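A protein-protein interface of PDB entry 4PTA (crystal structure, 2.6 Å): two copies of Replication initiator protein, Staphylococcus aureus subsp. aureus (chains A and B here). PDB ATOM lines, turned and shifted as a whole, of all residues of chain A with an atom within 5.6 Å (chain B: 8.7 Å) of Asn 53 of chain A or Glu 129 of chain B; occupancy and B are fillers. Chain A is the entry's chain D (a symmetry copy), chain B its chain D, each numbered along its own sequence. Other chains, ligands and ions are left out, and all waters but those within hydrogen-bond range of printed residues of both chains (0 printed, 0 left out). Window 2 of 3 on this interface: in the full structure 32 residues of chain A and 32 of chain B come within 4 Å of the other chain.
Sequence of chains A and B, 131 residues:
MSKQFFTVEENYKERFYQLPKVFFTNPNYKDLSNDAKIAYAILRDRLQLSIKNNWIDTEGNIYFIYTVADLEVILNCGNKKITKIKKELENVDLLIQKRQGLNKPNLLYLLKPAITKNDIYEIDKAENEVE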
ATOM      1  N   ARG A  46      -9.424 -25.420  24.413  1.00  0.00           N
ATOM      2  CA  ARG A  46      -8.381 -26.302  24.945  1.00  0.00           C
ATOM      3  C   ARG A  46      -6.983 -26.012  24.386  1.00  0.00           C
ATOM      4  O   ARG A  46      -6.004 -26.622  24.820  1.00  0.00           O
ATOM      5  CB  ARG A  46      -8.713 -27.775  24.675  1.00  0.00           C
ATOM      6  CG  ARG A  46     -10.195 -28.142  24.691  1.00  0.00           C
ATOM      7  CD  ARG A  46     -10.664 -28.541  26.078  1.00  0.00           C
ATOM      8  NE  ARG A  46      -9.761 -29.502  26.706  1.00  0.00           N
ATOM      9  CZ  ARG A  46      -9.950 -30.029  27.912  1.00  0.00           C
ATOM     10  NH1 ARG A  46     -11.017 -29.694  28.623  1.00  0.00           N
ATOM     11  NH2 ARG A  46      -9.072 -30.893  28.409  1.00  0.00           N
ATOM     12  N   GLN A  48      -4.775 -23.750  24.761  1.00  0.00           N
ATOM     13  CA  GLN A  48      -3.787 -23.351  25.752  1.00  0.00           C
ATOM     14  C   GLN A  48      -3.308 -24.554  26.561  1.00  0.00           C
ATOM     15  O   GLN A  48      -2.139 -24.637  26.938  1.00  0.00           O
ATOM     16  CB  GLN A  48      -4.384 -22.300  26.687  1.00  0.00           C
ATOM     17  CG  GLN A  48      -3.429 -21.186  27.064  1.00  0.00           C
ATOM     18  CD  GLN A  48      -3.763 -19.880  26.369  1.00  0.00           C
ATOM     19  OE1 GLN A  48      -3.956 -19.838  25.153  1.00  0.00           O
ATOM     20  NE2 GLN A  48      -3.845 -18.805  27.144  1.00  0.00           N
ATOM     21  N   LEU A  49      -4.220 -25.478  26.841  1.00  0.00           N
ATOM     22  CA  LEU A  49      -3.846 -26.722  27.496  1.00  0.00           C
ATOM     23  C   LEU A  49      -2.803 -27.447  26.652  1.00  0.00           C
ATOM     24  O   LEU A  49      -1.719 -27.764  27.134  1.00  0.00           O
ATOM     25  CB  LEU A  49      -5.069 -27.618  27.706  1.00  0.00           C
ATOM     26  CG  LEU A  49      -5.999 -27.305  28.877  1.00  0.00           C
ATOM     27  CD1 LEU A  49      -7.288 -28.100  28.766  1.00  0.00           C
ATOM     28  CD2 LEU A  49      -5.304 -27.581  30.199  1.00  0.00           C
ATOM     29  N   SER A  50      -3.130 -27.698  25.386  1.00  0.00           N
ATOM     30  CA  SER A  50      -2.248 -28.452  24.503  1.00  0.00           C
ATOM     31  C   SER A  50      -0.828 -27.900  24.519  1.00  0.00           C
ATOM     32  O   SER A  50       0.137 -28.658  24.506  1.00  0.00           O
ATOM     33  CB  SER A  50      -2.800 -28.481  23.077  1.00  0.00           C
ATOM     34  OG  SER A  50      -4.060 -29.128  23.036  1.00  0.00           O
ATOM     35  N   ILE A  51      -0.708 -26.577  24.548  1.00  0.00           N
ATOM     36  CA  ILE A  51       0.599 -25.932  24.630  1.00  0.00           C
ATOM     37  C   ILE A  51       1.334 -26.373  25.896  1.00  0.00           C
ATOM     38  O   ILE A  51       2.537 -26.635  25.870  1.00  0.00           O
ATOM     39  CB  ILE A  51       0.469 -24.397  24.612  1.00  0.00           C
ATOM     40  CG1 ILE A  51      -0.211 -23.939  23.321  1.00  0.00           C
ATOM     41  CG2 ILE A  51       1.834 -23.742  24.765  1.00  0.00           C
ATOM     42  CD1 ILE A  51      -0.448 -22.443  23.254  1.00  0.00           C
ATOM     43  N   LYS A  52       0.599 -26.455  26.999  1.00  0.00           N
ATOM     44  CA  LYS A  52       1.153 -26.915  28.268  1.00  0.00           C
ATOM     45  C   LYS A  52       1.558 -28.384  28.194  1.00  0.00           C
ATOM     46  O   LYS A  52       2.651 -28.755  28.621  1.00  0.00           O
ATOM     47  CB  LYS A  52       0.146 -26.702  29.399  1.00  0.00           C
ATOM     48  CG  LYS A  52       0.518 -27.390  30.697  1.00  0.00           C
ATOM     49  CD  LYS A  52      -0.653 -27.376  31.660  1.00  0.00           C
ATOM     50  CE  LYS A  52      -0.426 -28.321  32.822  1.00  0.00           C
ATOM     51  NZ  LYS A  52      -1.692 -28.553  33.576  1.00  0.00           N
ATOM     52  N   ASN A  53       0.675 -29.217  27.648  1.00  0.00           N
ATOM     53  CA  ASN A  53       0.989 -30.622  27.415  1.00  0.00           C
ATOM     54  C   ASN A  53       2.055 -30.769  26.333  1.00  0.00           C
ATOM     55  O   ASN A  53       2.390 -31.878  25.920  1.00  0.00           O
ATOM     56  CB  ASN A  53      -0.263 -31.405  27.012  1.00  0.00           C
ATOM     57  CG  ASN A  53      -1.346 -31.363  28.071  1.00  0.00           C
ATOM     58  OD1 ASN A  53      -1.095 -30.996  29.220  1.00  0.00           O
ATOM     59  ND2 ASN A  53      -2.562 -31.748  27.690  1.00  0.00           N
ATOM     60  N   ASN A  54       2.575 -29.636  25.876  1.00  0.00           N
ATOM     61  CA  ASN A  54       3.571 -29.603  24.812  1.00  0.00           C
ATOM     62  C   ASN A  54       3.108 -30.336  23.549  1.00  0.00           C
ATOM     63  O   ASN A  54       3.920 -30.853  22.781  1.00  0.00           O
ATOM     64  CB  ASN A  54       4.908 -30.155  25.311  1.00  0.00           C
ATOM     65  CG  ASN A  54       6.087 -29.628  24.515  1.00  0.00           C
ATOM     66  OD1 ASN A  54       6.545 -28.505  24.733  1.00  0.00           O
ATOM     67  ND2 ASN A  54       6.586 -30.439  23.588  1.00  0.00           N
ATOM     68  N   TRP A  55       1.794 -30.368  23.344  1.00  0.00           N
ATOM     69  CA  TRP A  55       1.213 -30.941  22.140  1.00  0.00           C
ATOM     70  C   TRP A  55       1.394 -29.992  20.968  1.00  0.00           C
ATOM     71  O   TRP A  55       0.422 -29.513  20.383  1.00  0.00           O
ATOM     72  CB  TRP A  55      -0.270 -31.237  22.354  1.00  0.00           C
ATOM     73  CG  TRP A  55      -0.513 -32.305  23.361  1.00  0.00           C
ATOM     74  CD1 TRP A  55       0.426 -33.074  23.980  1.00  0.00           C
ATOM     75  CD2 TRP A  55      -1.783 -32.726  23.880  1.00  0.00           C
ATOM     76  NE1 TRP A  55      -0.177 -33.950  24.849  1.00  0.00           N
ATOM     77  CE2 TRP A  55      -1.533 -33.754  24.805  1.00  0.00           C
ATOM     78  CE3 TRP A  55      -3.102 -32.330  23.645  1.00  0.00           C
ATOM     79  CZ2 TRP A  55      -2.554 -34.395  25.501  1.00  0.00           C
ATOM     80  CZ3 TRP A  55      -4.115 -32.970  24.338  1.00  0.00           C
ATOM     81  CH2 TRP A  55      -3.836 -33.989  25.253  1.00  0.00           C
ATOM     82  N   TYR A  66      -6.591 -37.077  22.204  1.00  0.00           N
ATOM     83  CA  TYR A  66      -7.781 -37.423  22.971  1.00  0.00           C
ATOM     84  C   TYR A  66      -8.387 -38.749  22.516  1.00  0.00           C
ATOM     85  O   TYR A  66      -8.552 -38.989  21.318  1.00  0.00           O
ATOM     86  CB  TYR A  66      -8.820 -36.302  22.866  1.00  0.00           C
ATOM     87  CG  TYR A  66      -8.438 -35.032  23.597  1.00  0.00           C
ATOM     88  CD1 TYR A  66      -8.807 -33.786  23.105  1.00  0.00           C
ATOM     89  CD2 TYR A  66      -7.719 -35.078  24.785  1.00  0.00           C
ATOM     90  CE1 TYR A  66      -8.466 -32.622  23.773  1.00  0.00           C
ATOM     91  CE2 TYR A  66      -7.371 -33.920  25.458  1.00  0.00           C
ATOM     92  CZ  TYR A  66      -7.748 -32.696  24.949  1.00  0.00           C
ATOM     93  OH  TYR A  66      -7.404 -31.543  25.616  1.00  0.00           O
ATOM     94  N   ASP B 124     -13.416 -25.507  36.681  1.00  0.00           N
ATOM     95  CA  ASP B 124     -11.985 -25.762  36.810  1.00  0.00           C
ATOM     96  C   ASP B 124     -11.626 -27.093  36.163  1.00  0.00           C
ATOM     97  O   ASP B 124     -10.673 -27.186  35.392  1.00  0.00           O
ATOM     98  CB  ASP B 124     -11.555 -25.780  38.278  1.00  0.00           C
ATOM     99  CG  ASP B 124     -11.614 -24.412  38.924  1.00  0.00           C
ATOM    100  OD1 ASP B 124     -10.781 -23.550  38.574  1.00  0.00           O
ATOM    101  OD2 ASP B 124     -12.481 -24.204  39.797  1.00  0.00           O
ATOM    102  N   LYS B 125     -12.394 -28.126  36.487  1.00  0.00           N
ATOM    103  CA  LYS B 125     -12.139 -29.449  35.944  1.00  0.00           C
ATOM    104  C   LYS B 125     -12.275 -29.430  34.421  1.00  0.00           C
ATOM    105  O   LYS B 125     -11.517 -30.092  33.711  1.00  0.00           O
ATOM    106  CB  LYS B 125     -13.087 -30.478  36.570  1.00  0.00           C
ATOM    107  CG  LYS B 125     -12.413 -31.781  37.005  1.00  0.00           C
ATOM    108  CD  LYS B 125     -11.673 -31.649  38.339  1.00  0.00           C
ATOM    109  CE  LYS B 125     -10.407 -30.809  38.224  1.00  0.00           C
ATOM    110  NZ  LYS B 125      -9.483 -31.315  37.169  1.00  0.00           N
ATOM    111  N   ALA B 126     -13.230 -28.646  33.932  1.00  0.00           N
ATOM    112  CA  ALA B 126     -13.492 -28.539  32.502  1.00  0.00           C
ATOM    113  C   ALA B 126     -12.407 -27.754  31.762  1.00  0.00           C
ATOM    114  O   ALA B 126     -12.234 -27.914  30.554  1.00  0.00           O
ATOM    115  CB  ALA B 126     -14.857 -27.909  32.265  1.00  0.00           C
ATOM    116  N   GLU B 127     -11.684 -26.906  32.485  1.00  0.00           N
ATOM    117  CA  GLU B 127     -10.654 -26.068  31.874  1.00  0.00           C
ATOM    118  C   GLU B 127      -9.251 -26.646  32.025  1.00  0.00           C
ATOM    119  O   GLU B 127      -8.283 -26.063  31.537  1.00  0.00           O
ATOM    120  CB  GLU B 127     -10.673 -24.661  32.473  1.00  0.00           C
ATOM    121  CG  GLU B 127     -11.836 -23.788  32.041  1.00  0.00           C
ATOM    122  CD  GLU B 127     -11.771 -22.409  32.671  1.00  0.00           C
ATOM    123  OE1 GLU B 127     -10.917 -22.207  33.559  1.00  0.00           O
ATOM    124  OE2 GLU B 127     -12.567 -21.528  32.281  1.00  0.00           O
ATOM    125  N   ASN B 128      -9.137 -27.782  32.705  1.00  0.00           N
ATOM    126  CA  ASN B 128      -7.828 -28.375  32.965  1.00  0.00           C
ATOM    127  C   ASN B 128      -7.668 -29.799  32.436  1.00  0.00           C
ATOM    128  O   ASN B 128      -8.620 -30.394  31.929  1.00  0.00           O
ATOM    129  CB  ASN B 128      -7.495 -28.316  34.459  1.00  0.00           C
ATOM    130  CG  ASN B 128      -7.149 -26.913  34.922  1.00  0.00           C
ATOM    131  OD1 ASN B 128      -6.000 -26.480  34.822  1.00  0.00           O
ATOM    132  ND2 ASN B 128      -8.144 -26.193  35.427  1.00  0.00           N
ATOM    133  N   GLU B 129      -6.449 -30.324  32.552  1.00  0.00           N
ATOM    134  CA  GLU B 129      -6.107 -31.669  32.086  1.00  0.00           C
ATOM    135  C   GLU B 129      -7.222 -32.684  32.331  1.00  0.00           C
ATOM    136  O   GLU B 129      -7.891 -32.648  33.364  1.00  0.00           O
ATOM    137  CB  GLU B 129      -4.824 -32.152  32.771  1.00  0.00           C
ATOM    138  CG  GLU B 129      -3.655 -32.419  31.833  1.00  0.00           C
ATOM    139  CD  GLU B 129      -3.017 -31.145  31.313  1.00  0.00           C
ATOM    140  OE1 GLU B 129      -3.662 -30.442  30.507  1.00  0.00           O
ATOM    141  OE2 GLU B 129      -1.869 -30.849  31.710  1.00  0.00           O
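OE2 of Glu 129 of chain B lies close to OD1 of Asn 53 of chain A, 2.6 Å away. The side-chain carboxylate (OE2) of Glu 129 of chain B lies within salt-bridge range of the side-chain amino group (NZ) of Lys 52 of chain A (3.0 Å). The backbone carbonyl oxygen of Ala 126 of chain B sits at hydrogen-bond distance from the guanidinium group of Arg 46 of chain A.
The backbone carbonyl oxygen (O) of Asp 124 of chain B sits at hydrogen-bond distance from the side-chain amide nitrogen (ND2) of Asn 128 of chain B (2.7 Å). The side-chain hydroxyl (OH) of Tyr 66 of chain A is in hydrogen-bond range of the guanidinium group (NE) of Arg 46 of chain A. The indole nitrogen of Trp 55 of chain A lies close to the backbone carbonyl oxygen of Asn 53 of chain A (3.5 Å).
Among the printed residues, pairs that only touch across the chains: Leu 49 of chain A with Glu 129 of chain B (3.3 Å), Leu 49 of chain A with Glu 127 of chain B (3.6 Å), Arg 46 of chain A with Asn 128 of chain B (3.6 Å) and Leu 49 of chain A with Asn 128 of chain B (3.8 Å).
Of the printed residues of chain B, Arg 46 of chain A touches Ala 126 and Asn 128. Printed residues of chain B within 4 Å of Leu 49 of chain A: Glu 127, Asn 128 and Glu 129. Of chain B, only Glu 129 comes within 4 Å of Asn 53 of chain A. Lys 125 of chain B touches none of the printed residues of chain A. Printed residues of chain A within 4 Å of Glu 127 of chain B: Leu 49. Of the printed residues of chain A, Asn 128 of chain B touches Arg 46 (3.6 Å) and Leu 49 (3.8 Å). Glu 129 of chain B touches three residues of chain A. The nearest residue of chain A that does not touch Glu 129 of chain B is Arg 46 of chain A (4.7 Å). The nearest printed residue of chain B that does not touch Leu 49 of chain A is Ala 126 of chain B (5.3 Å).
Printed residues of chain A that touch a printed residue of chain B: Arg 46, Leu 49, Lys 52 and Asn 53. Among the printed residues, 7 pairs touch across the chains.
No position is printed for both chains.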
